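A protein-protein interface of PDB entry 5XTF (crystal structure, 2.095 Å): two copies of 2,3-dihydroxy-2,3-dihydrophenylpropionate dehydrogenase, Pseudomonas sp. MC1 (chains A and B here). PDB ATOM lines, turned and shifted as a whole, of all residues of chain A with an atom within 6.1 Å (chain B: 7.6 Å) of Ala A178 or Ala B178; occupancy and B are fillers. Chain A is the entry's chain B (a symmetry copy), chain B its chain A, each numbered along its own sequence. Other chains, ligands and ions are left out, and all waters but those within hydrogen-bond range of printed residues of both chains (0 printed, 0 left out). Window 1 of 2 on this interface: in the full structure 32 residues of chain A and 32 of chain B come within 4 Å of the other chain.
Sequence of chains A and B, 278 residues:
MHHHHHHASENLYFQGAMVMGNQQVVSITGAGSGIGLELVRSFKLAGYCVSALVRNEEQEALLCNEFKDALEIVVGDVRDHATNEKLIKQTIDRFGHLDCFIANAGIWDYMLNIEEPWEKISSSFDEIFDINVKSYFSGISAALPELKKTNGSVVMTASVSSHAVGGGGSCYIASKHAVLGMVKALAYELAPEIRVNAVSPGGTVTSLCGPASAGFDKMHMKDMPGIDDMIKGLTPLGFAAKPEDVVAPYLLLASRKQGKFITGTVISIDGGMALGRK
Phe B129 touches its own counterpart, Phe A129.
Ile A173 touches Gly B181, and with the chains exchanged Gly A181 touches Ile B173.
His A177 touches its own counterpart, His B177.
Ala B178 touches its own counterpart, Ala A178.
13 positions are printed for both chains.
Of the 14 pairs that touch across the chains among the printed residues, 11 have their exchanged pair printed and touching as well.
The side-chain amino group (NZ) of Lys B184 is in hydrogen-bond range of a ring nitrogen (NE2) of His A177, 3.0 Å away.
Of chain B, only Ala B174 (3.4 Å) and Ala B178 (3.9 Å) come within 4 Å of Ala A178.
Ala B178 touches two residues of chain A.
Printed residues of chain B within 4 Å of Ala A174: Ala B178 (3.3 Å) and Met B182 (3.99 Å).
Of the printed residues of chain B, Met A182 touches Ala B174.
Printed residues of chain A within 4 Å of Lys B184: His A177.
Of the printed residues of chain A, Ala B185 touches Ile A173 (3.9 Å).
Phe A129 touches Phe B129.
CG1 of Val A133 touches CE1 of Phe B125 (3.7 Å).
CB of Ala B185 touches CD1 of Ile A173 (3.9 Å).
CB of Ala B178 touches O of Ala A174, at 3.3 Å.
O of His A177 touches CB of His B177, 3.3 Å away.
CG of His A177 touches CA of Gly B181 (3.5 Å).
O of Ala B174 touches CB of Ala A178, 3.4 Å away.
Ala A178 touches Ala B178 (CB to CB, 3.9 Å).
Gly A181 touches Ile B173 (O to CG2, 3.8 Å).
Ala B174 touches Met A182 (CB to CG, 3.8 Å).
Of the 25 printed residues of chain B, 10 touch a printed residue of chain A.
Hydrophobic or aromatic side chains of chain B within 4 Å of the printed part of chain A: Phe B125, Phe B129, Ile B173, Ala B174, His B177, Ala B178, Met B182 and Ala B185.
Hydrophobic or aromatic side chains of chain A within 4 Å of the printed part of chain B: Phe A129, Val A133, Ile A173, Ala A174, His A177, Ala A178 and Met A182.
Among the printed residues, 14 pairs touch across the chains.
Among the printed residues, no Asp or Glu carboxylate lies within 4 Å of a Lys or Arg side-chain nitrogen of the other chain.
The backbone carbonyl oxygen (O) of Ile A173 is in hydrogen-bond range of a ring nitrogen (ND1) of His A177 (2.8 Å).
A ring nitrogen (ND1) of His B177 is in hydrogen-bond range of the backbone carbonyl oxygen (O) of Ile B173 (2.8 Å).
O of Ser B162 is in hydrogen-bond range of NE2 of His B177, 2.9 Å away.
O of Ser B161 sits close to ND1 of His B177 (3.2 Å).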
ATOM      1  N   PHE A 129     -30.491   9.913  13.857  1.00  0.00           N
ATOM      2  CA  PHE A 129     -29.146   9.831  13.306  1.00  0.00           C
ATOM      3  C   PHE A 129     -29.145   9.600  11.796  1.00  0.00           C
ATOM      4  O   PHE A 129     -28.233  10.080  11.105  1.00  0.00           O
ATOM      5  CB  PHE A 129     -28.351   8.766  14.053  1.00  0.00           C
ATOM      6  CG  PHE A 129     -27.758   9.283  15.337  1.00  0.00           C
ATOM      7  CD1 PHE A 129     -28.545   9.448  16.461  1.00  0.00           C
ATOM      8  CD2 PHE A 129     -26.415   9.657  15.398  1.00  0.00           C
ATOM      9  CE1 PHE A 129     -27.999   9.960  17.636  1.00  0.00           C
ATOM     10  CE2 PHE A 129     -25.862  10.173  16.565  1.00  0.00           C
ATOM     11  CZ  PHE A 129     -26.659  10.314  17.689  1.00  0.00           C
ATOM     12  N   VAL A 133     -27.482  13.114  10.724  1.00  0.00           N
ATOM     13  CA  VAL A 133     -26.066  12.797  10.587  1.00  0.00           C
ATOM     14  C   VAL A 133     -25.791  11.961   9.347  1.00  0.00           C
ATOM     15  O   VAL A 133     -25.025  12.378   8.474  1.00  0.00           O
ATOM     16  CB  VAL A 133     -25.522  12.079  11.834  1.00  0.00           C
ATOM     17  CG1 VAL A 133     -24.017  11.816  11.672  1.00  0.00           C
ATOM     18  CG2 VAL A 133     -25.809  12.893  13.104  1.00  0.00           C
ATOM     19  N   ILE A 173     -29.301  16.017  20.947  1.00  0.00           N
ATOM     20  CA  ILE A 173     -28.072  16.718  21.293  1.00  0.00           C
ATOM     21  C   ILE A 173     -26.859  15.928  20.829  1.00  0.00           C
ATOM     22  O   ILE A 173     -25.877  16.503  20.341  1.00  0.00           O
ATOM     23  CB  ILE A 173     -28.028  17.021  22.799  1.00  0.00           C
ATOM     24  CG1 ILE A 173     -29.080  18.075  23.125  1.00  0.00           C
ATOM     25  CG2 ILE A 173     -26.661  17.523  23.192  1.00  0.00           C
ATOM     26  CD1 ILE A 173     -29.148  18.454  24.554  1.00  0.00           C
ATOM     27  N   ALA A 174     -26.926  14.597  20.930  1.00  0.00           N
ATOM     28  CA  ALA A 174     -25.821  13.767  20.462  1.00  0.00           C
ATOM     29  C   ALA A 174     -25.674  13.855  18.947  1.00  0.00           C
ATOM     30  O   ALA A 174     -24.554  13.904  18.429  1.00  0.00           O
ATOM     31  CB  ALA A 174     -26.035  12.323  20.911  1.00  0.00           C
ATOM     32  N   SER A 175     -26.790  13.892  18.216  1.00  0.00           N
ATOM     33  CA  SER A 175     -26.684  13.995  16.763  1.00  0.00           C
ATOM     34  C   SER A 175     -26.102  15.343  16.357  1.00  0.00           C
ATOM     35  O   SER A 175     -25.294  15.427  15.429  1.00  0.00           O
ATOM     36  CB  SER A 175     -28.043  13.782  16.093  1.00  0.00           C
ATOM     37  OG  SER A 175     -28.927  14.880  16.274  1.00  0.00           O
ATOM     38  N   LYS A 176     -26.486  16.401  17.050  1.00  0.00           N
ATOM     39  CA  LYS A 176     -25.962  17.713  16.703  1.00  0.00           C
ATOM     40  C   LYS A 176     -24.504  17.868  17.107  1.00  0.00           C
ATOM     41  O   LYS A 176     -23.767  18.618  16.461  1.00  0.00           O
ATOM     42  CB  LYS A 176     -26.848  18.783  17.329  1.00  0.00           C
ATOM     43  CG  LYS A 176     -28.205  18.884  16.577  1.00  0.00           C
ATOM     44  CD  LYS A 176     -27.978  19.208  15.083  1.00  0.00           C
ATOM     45  CE  LYS A 176     -29.284  19.450  14.346  1.00  0.00           C
ATOM     46  NZ  LYS A 176     -29.024  19.837  12.922  1.00  0.00           N
ATOM     47  N   HIS A 177     -24.053  17.157  18.148  1.00  0.00           N
ATOM     48  CA  HIS A 177     -22.620  17.123  18.415  1.00  0.00           C
ATOM     49  C   HIS A 177     -21.867  16.343  17.348  1.00  0.00           C
ATOM     50  O   HIS A 177     -20.753  16.721  16.967  1.00  0.00           O
ATOM     51  CB  HIS A 177     -22.351  16.539  19.795  1.00  0.00           C
ATOM     52  CG  HIS A 177     -22.492  17.535  20.897  1.00  0.00           C
ATOM     53  ND1 HIS A 177     -23.719  18.000  21.326  1.00  0.00           N
ATOM     54  CD2 HIS A 177     -21.561  18.165  21.652  1.00  0.00           C
ATOM     55  CE1 HIS A 177     -23.535  18.871  22.302  1.00  0.00           C
ATOM     56  NE2 HIS A 177     -22.236  18.987  22.520  1.00  0.00           N
ATOM     57  N   ALA A 178     -22.448  15.251  16.850  1.00  0.00           N
ATOM     58  CA  ALA A 178     -21.795  14.527  15.766  1.00  0.00           C
ATOM     59  C   ALA A 178     -21.561  15.433  14.553  1.00  0.00           C
ATOM     60  O   ALA A 178     -20.517  15.341  13.899  1.00  0.00           O
ATOM     61  CB  ALA A 178     -22.614  13.288  15.396  1.00  0.00           C
ATOM     62  N   VAL A 179     -22.496  16.350  14.262  1.00  0.00           N
ATOM     63  CA  VAL A 179     -22.299  17.259  13.125  1.00  0.00           C
ATOM     64  C   VAL A 179     -21.055  18.126  13.334  1.00  0.00           C
ATOM     65  O   VAL A 179     -20.239  18.290  12.418  1.00  0.00           O
ATOM     66  CB  VAL A 179     -23.556  18.120  12.868  1.00  0.00           C
ATOM     67  CG1 VAL A 179     -23.322  19.036  11.710  1.00  0.00           C
ATOM     68  CG2 VAL A 179     -24.777  17.223  12.581  1.00  0.00           C
ATOM     69  N   LEU A 180     -20.861  18.651  14.549  1.00  0.00           N
ATOM     70  CA  LEU A 180     -19.609  19.341  14.861  1.00  0.00           C
ATOM     71  C   LEU A 180     -18.409  18.479  14.540  1.00  0.00           C
ATOM     72  O   LEU A 180     -17.386  18.982  14.067  1.00  0.00           O
ATOM     73  CB  LEU A 180     -19.541  19.718  16.333  1.00  0.00           C
ATOM     74  CG  LEU A 180     -20.574  20.677  16.886  1.00  0.00           C
ATOM     75  CD1 LEU A 180     -20.116  21.067  18.287  1.00  0.00           C
ATOM     76  CD2 LEU A 180     -20.715  21.888  15.993  1.00  0.00           C
ATOM     77  N   GLY A 181     -18.506  17.178  14.812  1.00  0.00           N
ATOM     78  CA  GLY A 181     -17.391  16.296  14.529  1.00  0.00           C
ATOM     79  C   GLY A 181     -17.126  16.176  13.043  1.00  0.00           C
ATOM     80  O   GLY A 181     -15.973  16.219  12.605  1.00  0.00           O
ATOM     81  N   MET A 182     -18.191  16.035  12.252  1.00  0.00           N
ATOM     82  CA  MET A 182     -18.061  15.998  10.796  1.00  0.00           C
ATOM     83  C   MET A 182     -17.402  17.255  10.255  1.00  0.00           C
ATOM     84  O   MET A 182     -16.552  17.178   9.363  1.00  0.00           O
ATOM     85  CB  MET A 182     -19.429  15.833  10.141  1.00  0.00           C
ATOM     86  CG  MET A 182     -20.203  14.632  10.554  1.00  0.00           C
ATOM     87  SD  MET A 182     -21.822  14.658   9.736  1.00  0.00           S
ATOM     88  CE  MET A 182     -21.364  14.485   8.008  1.00  0.00           C
ATOM     89  N   VAL A 183     -17.822  18.427  10.742  1.00  0.00           N
ATOM     90  CA  VAL A 183     -17.261  19.692  10.267  1.00  0.00           C
ATOM     91  C   VAL A 183     -15.749  19.705  10.437  1.00  0.00           C
ATOM     92  O   VAL A 183     -15.008  20.103   9.533  1.00  0.00           O
ATOM     93  CB  VAL A 183     -17.900  20.889  10.995  1.00  0.00           C
ATOM     94  CG1 VAL A 183     -17.172  22.136  10.627  1.00  0.00           C
ATOM     95  CG2 VAL A 183     -19.364  21.022  10.650  1.00  0.00           C
ATOM     96  N   PHE B 125     -20.389   3.320   8.558  1.00  0.00           N
ATOM     97  CA  PHE B 125     -21.114   4.238   9.443  1.00  0.00           C
ATOM     98  C   PHE B 125     -22.068   3.482  10.362  1.00  0.00           C
ATOM     99  O   PHE B 125     -22.151   3.773  11.559  1.00  0.00           O
ATOM    100  CB  PHE B 125     -21.887   5.280   8.615  1.00  0.00           C
ATOM    101  CG  PHE B 125     -22.789   6.204   9.435  1.00  0.00           C
ATOM    102  CD1 PHE B 125     -22.414   7.520   9.688  1.00  0.00           C
ATOM    103  CD2 PHE B 125     -24.022   5.767   9.924  1.00  0.00           C
ATOM    104  CE1 PHE B 125     -23.235   8.370  10.434  1.00  0.00           C
ATOM    105  CE2 PHE B 125     -24.829   6.604  10.670  1.00  0.00           C
ATOM    106  CZ  PHE B 125     -24.435   7.905  10.923  1.00  0.00           C
ATOM    107  N   PHE B 129     -21.482   3.726  14.297  1.00  0.00           N
ATOM    108  CA  PHE B 129     -22.440   4.413  15.156  1.00  0.00           C
ATOM    109  C   PHE B 129     -23.230   3.443  16.031  1.00  0.00           C
ATOM    110  O   PHE B 129     -23.545   3.778  17.185  1.00  0.00           O
ATOM    111  CB  PHE B 129     -23.349   5.306  14.308  1.00  0.00           C
ATOM    112  CG  PHE B 129     -22.814   6.696  14.146  1.00  0.00           C
ATOM    113  CD1 PHE B 129     -21.740   6.944  13.310  1.00  0.00           C
ATOM    114  CD2 PHE B 129     -23.358   7.747  14.863  1.00  0.00           C
ATOM    115  CE1 PHE B 129     -21.224   8.228  13.179  1.00  0.00           C
ATOM    116  CE2 PHE B 129     -22.850   9.041  14.746  1.00  0.00           C
ATOM    117  CZ  PHE B 129     -21.782   9.277  13.901  1.00  0.00           C
ATOM    118  N   ASN B 132     -20.367   2.614  18.830  1.00  0.00           N
ATOM    119  CA  ASN B 132     -19.804   3.740  19.578  1.00  0.00           C
ATOM    120  C   ASN B 132     -20.849   4.669  20.181  1.00  0.00           C
ATOM    121  O   ASN B 132     -20.512   5.433  21.083  1.00  0.00           O
ATOM    122  CB  ASN B 132     -18.874   4.562  18.676  1.00  0.00           C
ATOM    123  CG  ASN B 132     -17.590   3.827  18.351  1.00  0.00           C
ATOM    124  OD1 ASN B 132     -17.335   2.747  18.898  1.00  0.00           O
ATOM    125  ND2 ASN B 132     -16.781   4.391  17.457  1.00  0.00           N
ATOM    126  N   VAL B 133     -22.094   4.653  19.700  1.00  0.00           N
ATOM    127  CA  VAL B 133     -23.080   5.598  20.209  1.00  0.00           C
ATOM    128  C   VAL B 133     -24.359   4.894  20.645  1.00  0.00           C
ATOM    129  O   VAL B 133     -24.803   5.069  21.784  1.00  0.00           O
ATOM    130  CB  VAL B 133     -23.412   6.685  19.170  1.00  0.00           C
ATOM    131  CG1 VAL B 133     -24.364   7.715  19.778  1.00  0.00           C
ATOM    132  CG2 VAL B 133     -22.137   7.325  18.620  1.00  0.00           C
ATOM    133  N   TYR B 136     -24.203   2.794  23.737  1.00  0.00           N
ATOM    134  CA  TYR B 136     -24.122   3.488  25.021  1.00  0.00           C
ATOM    135  C   TYR B 136     -25.514   3.845  25.514  1.00  0.00           C
ATOM    136  O   TYR B 136     -25.843   3.636  26.691  1.00  0.00           O
ATOM    137  CB  TYR B 136     -23.259   4.751  24.924  1.00  0.00           C
ATOM    138  CG  TYR B 136     -21.756   4.557  24.839  1.00  0.00           C
ATOM    139  CD1 TYR B 136     -21.176   3.301  24.641  1.00  0.00           C
ATOM    140  CD2 TYR B 136     -20.908   5.651  24.965  1.00  0.00           C
ATOM    141  CE1 TYR B 136     -19.759   3.154  24.573  1.00  0.00           C
ATOM    142  CE2 TYR B 136     -19.515   5.523  24.891  1.00  0.00           C
ATOM    143  CZ  TYR B 136     -18.943   4.290  24.701  1.00  0.00           C
ATOM    144  OH  TYR B 136     -17.556   4.233  24.640  1.00  0.00           O
ATOM    145  N   PHE B 137     -26.352   4.383  24.621  1.00  0.00           N
ATOM    146  CA  PHE B 137     -27.750   4.580  24.962  1.00  0.00           C
ATOM    147  C   PHE B 137     -28.368   3.279  25.465  1.00  0.00           C
ATOM    148  O   PHE B 137     -29.101   3.273  26.460  1.00  0.00           O
ATOM    149  CB  PHE B 137     -28.520   5.095  23.745  1.00  0.00           C
ATOM    150  CG  PHE B 137     -28.394   6.577  23.518  1.00  0.00           C
ATOM    151  CD1 PHE B 137     -27.555   7.080  22.532  1.00  0.00           C
ATOM    152  CD2 PHE B 137     -29.122   7.466  24.283  1.00  0.00           C
ATOM    153  CE1 PHE B 137     -27.452   8.448  22.312  1.00  0.00           C
ATOM    154  CE2 PHE B 137     -29.028   8.829  24.064  1.00  0.00           C
ATOM    155  CZ  PHE B 137     -28.187   9.318  23.081  1.00  0.00           C
ATOM    156  N   MET B 156     -18.597   7.070  30.472  1.00  0.00           N
ATOM    157  CA  MET B 156     -18.446   6.679  29.081  1.00  0.00           C
ATOM    158  C   MET B 156     -17.003   6.841  28.633  1.00  0.00           C
ATOM    159  O   MET B 156     -16.291   7.734  29.097  1.00  0.00           O
ATOM    160  CB  MET B 156     -19.358   7.522  28.187  1.00  0.00           C
ATOM    161  CG  MET B 156     -20.812   7.083  28.266  1.00  0.00           C
ATOM    162  SD  MET B 156     -21.959   8.171  27.411  1.00  0.00           S
ATOM    163  CE  MET B 156     -22.433   9.258  28.740  1.00  0.00           C
ATOM    164  N   SER B 161     -10.300  11.752  19.642  1.00  0.00           N
ATOM    165  CA  SER B 161     -11.095  12.088  18.467  1.00  0.00           C
ATOM    166  C   SER B 161     -12.404  12.777  18.813  1.00  0.00           C
ATOM    167  O   SER B 161     -13.093  13.245  17.899  1.00  0.00           O
ATOM    168  CB  SER B 161     -11.388  10.826  17.641  1.00  0.00           C
ATOM    169  OG  SER B 161     -10.207  10.313  17.050  1.00  0.00           O
ATOM    170  N   SER B 162     -12.787  12.832  20.091  1.00  0.00           N
ATOM    171  CA  SER B 162     -13.923  13.663  20.468  1.00  0.00           C
ATOM    172  C   SER B 162     -13.581  15.149  20.429  1.00  0.00           C
ATOM    173  O   SER B 162     -14.496  15.979  20.419  1.00  0.00           O
ATOM    174  CB  SER B 162     -14.423  13.299  21.870  1.00  0.00           C
ATOM    175  OG  SER B 162     -14.698  11.915  21.998  1.00  0.00           O
ATOM    176  N   SER B 170     -13.764  10.458   9.304  1.00  0.00           N
ATOM    177  CA  SER B 170     -14.875  11.320   9.687  1.00  0.00           C
ATOM    178  C   SER B 170     -15.954  10.557  10.461  1.00  0.00           C
ATOM    179  O   SER B 170     -16.543  11.098  11.404  1.00  0.00           O
ATOM    180  CB  SER B 170     -15.452  11.996   8.446  1.00  0.00           C
ATOM    181  OG  SER B 170     -15.507  11.094   7.348  1.00  0.00           O
ATOM    182  N   CYS B 171     -16.228   9.296  10.090  1.00  0.00           N
ATOM    183  CA  CYS B 171     -17.243   8.538  10.827  1.00  0.00           C
ATOM    184  C   CYS B 171     -16.850   8.373  12.288  1.00  0.00           C
ATOM    185  O   CYS B 171     -17.662   8.580  13.198  1.00  0.00           O
ATOM    186  CB  CYS B 171     -17.458   7.168  10.193  1.00  0.00           C
ATOM    187  SG  CYS B 171     -18.211   7.249   8.575  1.00  0.00           S
ATOM    188  N   TYR B 172     -15.604   7.978  12.530  1.00  0.00           N
ATOM    189  CA  TYR B 172     -15.160   7.779  13.899  1.00  0.00           C
ATOM    190  C   TYR B 172     -15.173   9.091  14.663  1.00  0.00           C
ATOM    191  O   TYR B 172     -15.696   9.167  15.779  1.00  0.00           O
ATOM    192  CB  TYR B 172     -13.765   7.157  13.911  1.00  0.00           C
ATOM    193  CG  TYR B 172     -13.227   6.867  15.297  1.00  0.00           C
ATOM    194  CD1 TYR B 172     -13.652   5.741  16.009  1.00  0.00           C
ATOM    195  CD2 TYR B 172     -12.278   7.702  15.896  1.00  0.00           C
ATOM    196  CE1 TYR B 172     -13.159   5.456  17.285  1.00  0.00           C
ATOM    197  CE2 TYR B 172     -11.772   7.413  17.186  1.00  0.00           C
ATOM    198  CZ  TYR B 172     -12.221   6.284  17.869  1.00  0.00           C
ATOM    199  OH  TYR B 172     -11.743   5.984  19.135  1.00  0.00           O
ATOM    200  N   ILE B 173     -14.597  10.142  14.076  1.00  0.00           N
ATOM    201  CA  ILE B 173     -14.517  11.417  14.783  1.00  0.00           C
ATOM    202  C   ILE B 173     -15.908  11.934  15.111  1.00  0.00           C
ATOM    203  O   ILE B 173     -16.141  12.476  16.195  1.00  0.00           O
ATOM    204  CB  ILE B 173     -13.703  12.431  13.971  1.00  0.00           C
ATOM    205  CG1 ILE B 173     -12.236  12.033  14.015  1.00  0.00           C
ATOM    206  CG2 ILE B 173     -13.860  13.809  14.561  1.00  0.00           C
ATOM    207  CD1 ILE B 173     -11.350  12.827  13.082  1.00  0.00           C
ATOM    208  N   ALA B 174     -16.871  11.727  14.203  1.00  0.00           N
ATOM    209  CA  ALA B 174     -18.235  12.178  14.472  1.00  0.00           C
ATOM    210  C   ALA B 174     -18.901  11.316  15.543  1.00  0.00           C
ATOM    211  O   ALA B 174     -19.676  11.821  16.359  1.00  0.00           O
ATOM    212  CB  ALA B 174     -19.060  12.181  13.183  1.00  0.00           C
ATOM    213  N   SER B 175     -18.627  10.015  15.556  1.00  0.00           N
ATOM    214  CA  SER B 175     -19.206   9.191  16.621  1.00  0.00           C
ATOM    215  C   SER B 175     -18.645   9.583  17.984  1.00  0.00           C
ATOM    216  O   SER B 175     -19.361   9.584  18.989  1.00  0.00           O
ATOM    217  CB  SER B 175     -18.937   7.709  16.363  1.00  0.00           C
ATOM    218  OG  SER B 175     -17.582   7.391  16.642  1.00  0.00           O
ATOM    219  N   LYS B 176     -17.367   9.925  18.040  1.00  0.00           N
ATOM    220  CA  LYS B 176     -16.800  10.302  19.324  1.00  0.00           C
ATOM    221  C   LYS B 176     -17.281  11.677  19.777  1.00  0.00           C
ATOM    222  O   LYS B 176     -17.391  11.920  20.980  1.00  0.00           O
ATOM    223  CB  LYS B 176     -15.285  10.205  19.235  1.00  0.00           C
ATOM    224  CG  LYS B 176     -14.851   8.709  19.201  1.00  0.00           C
ATOM    225  CD  LYS B 176     -15.516   7.934  20.356  1.00  0.00           C
ATOM    226  CE  LYS B 176     -14.843   6.603  20.637  1.00  0.00           C
ATOM    227  NZ  LYS B 176     -15.321   6.025  21.934  1.00  0.00           N
ATOM    228  N   HIS B 177     -17.620  12.571  18.842  1.00  0.00           N
ATOM    229  CA  HIS B 177     -18.243  13.828  19.244  1.00  0.00           C
ATOM    230  C   HIS B 177     -19.651  13.607  19.768  1.00  0.00           C
ATOM    231  O   HIS B 177     -20.085  14.282  20.710  1.00  0.00           O
ATOM    232  CB  HIS B 177     -18.263  14.819  18.079  1.00  0.00           C
ATOM    233  CG  HIS B 177     -16.979  15.557  17.901  1.00  0.00           C
ATOM    234  ND1 HIS B 177     -15.825  14.944  17.459  1.00  0.00           N
ATOM    235  CD2 HIS B 177     -16.663  16.859  18.109  1.00  0.00           C
ATOM    236  CE1 HIS B 177     -14.852  15.835  17.408  1.00  0.00           C
ATOM    237  NE2 HIS B 177     -15.335  17.005  17.794  1.00  0.00           N
ATOM    238  N   ALA B 178     -20.398  12.688  19.158  1.00  0.00           N
ATOM    239  CA  ALA B 178     -21.738  12.418  19.661  1.00  0.00           C
ATOM    240  C   ALA B 178     -21.699  11.971  21.123  1.00  0.00           C
ATOM    241  O   ALA B 178     -22.567  12.348  21.920  1.00  0.00           O
ATOM    242  CB  ALA B 178     -22.421  11.375  18.775  1.00  0.00           C
ATOM    243  N   VAL B 179     -20.689  11.180  21.500  1.00  0.00           N
ATOM    244  CA  VAL B 179     -20.558  10.771  22.897  1.00  0.00           C
ATOM    245  C   VAL B 179     -20.385  11.994  23.801  1.00  0.00           C
ATOM    246  O   VAL B 179     -20.929  12.042  24.908  1.00  0.00           O
ATOM    247  CB  VAL B 179     -19.404   9.757  23.057  1.00  0.00           C
ATOM    248  CG1 VAL B 179     -19.145   9.437  24.539  1.00  0.00           C
ATOM    249  CG2 VAL B 179     -19.723   8.476  22.296  1.00  0.00           C
ATOM    250  N   LEU B 180     -19.666  13.017  23.336  1.00  0.00           N
ATOM    251  CA  LEU B 180     -19.548  14.225  24.151  1.00  0.00           C
ATOM    252  C   LEU B 180     -20.905  14.854  24.370  1.00  0.00           C
ATOM    253  O   LEU B 180     -21.168  15.419  25.433  1.00  0.00           O
ATOM    254  CB  LEU B 180     -18.636  15.252  23.498  1.00  0.00           C
ATOM    255  CG  LEU B 180     -17.165  14.947  23.348  1.00  0.00           C
ATOM    256  CD1 LEU B 180     -16.479  16.190  22.796  1.00  0.00           C
ATOM    257  CD2 LEU B 180     -16.604  14.586  24.679  1.00  0.00           C
ATOM    258  N   GLY B 181     -21.778  14.771  23.365  1.00  0.00           N
ATOM    259  CA  GLY B 181     -23.109  15.327  23.513  1.00  0.00           C
ATOM    260  C   GLY B 181     -23.945  14.506  24.469  1.00  0.00           C
ATOM    261  O   GLY B 181     -24.742  15.051  25.239  1.00  0.00           O
ATOM    262  N   MET B 182     -23.780  13.178  24.421  1.00  0.00           N
ATOM    263  CA  MET B 182     -24.408  12.302  25.408  1.00  0.00           C
ATOM    264  C   MET B 182     -24.066  12.732  26.820  1.00  0.00           C
ATOM    265  O   MET B 182     -24.944  12.800  27.681  1.00  0.00           O
ATOM    266  CB  MET B 182     -23.966  10.856  25.201  1.00  0.00           C
ATOM    267  CG  MET B 182     -24.444  10.260  23.931  1.00  0.00           C
ATOM    268  SD  MET B 182     -24.196   8.479  23.928  1.00  0.00           S
ATOM    269  CE  MET B 182     -25.336   7.984  25.215  1.00  0.00           C
ATOM    270  N   VAL B 183     -22.780  12.999  27.084  1.00  0.00           N
ATOM    271  CA  VAL B 183     -22.367  13.298  28.454  1.00  0.00           C
ATOM    272  C   VAL B 183     -23.087  14.534  28.959  1.00  0.00           C
ATOM    273  O   VAL B 183     -23.608  14.554  30.079  1.00  0.00           O
ATOM    274  CB  VAL B 183     -20.839  13.464  28.558  1.00  0.00           C
ATOM    275  CG1 VAL B 183     -20.469  13.917  29.948  1.00  0.00           C
ATOM    276  CG2 VAL B 183     -20.126  12.169  28.232  1.00  0.00           C
ATOM    277  N   LYS B 184     -23.135  15.580  28.140  1.00  0.00           N
ATOM    278  CA  LYS B 184     -23.710  16.828  28.615  1.00  0.00           C
ATOM    279  C   LYS B 184     -25.219  16.720  28.749  1.00  0.00           C
ATOM    280  O   LYS B 184     -25.793  17.182  29.742  1.00  0.00           O
ATOM    281  CB  LYS B 184     -23.301  17.968  27.683  1.00  0.00           C
ATOM    282  CG  LYS B 184     -21.768  18.099  27.616  1.00  0.00           C
ATOM    283  CD  LYS B 184     -21.314  18.620  26.263  1.00  0.00           C
ATOM    284  CE  LYS B 184     -21.257  20.135  26.240  1.00  0.00           C
ATOM    285  NZ  LYS B 184     -21.236  20.668  24.858  1.00  0.00           N
ATOM    286  N   ALA B 185     -25.875  16.086  27.773  1.00  0.00           N
ATOM    287  CA  ALA B 185     -27.325  15.923  27.816  1.00  0.00           C
ATOM    288  C   ALA B 185     -27.758  15.030  28.978  1.00  0.00           C
ATOM    289  O   ALA B 185     -28.677  15.376  29.727  1.00  0.00           O
ATOM    290  CB  ALA B 185     -27.816  15.351  26.483  1.00  0.00           C
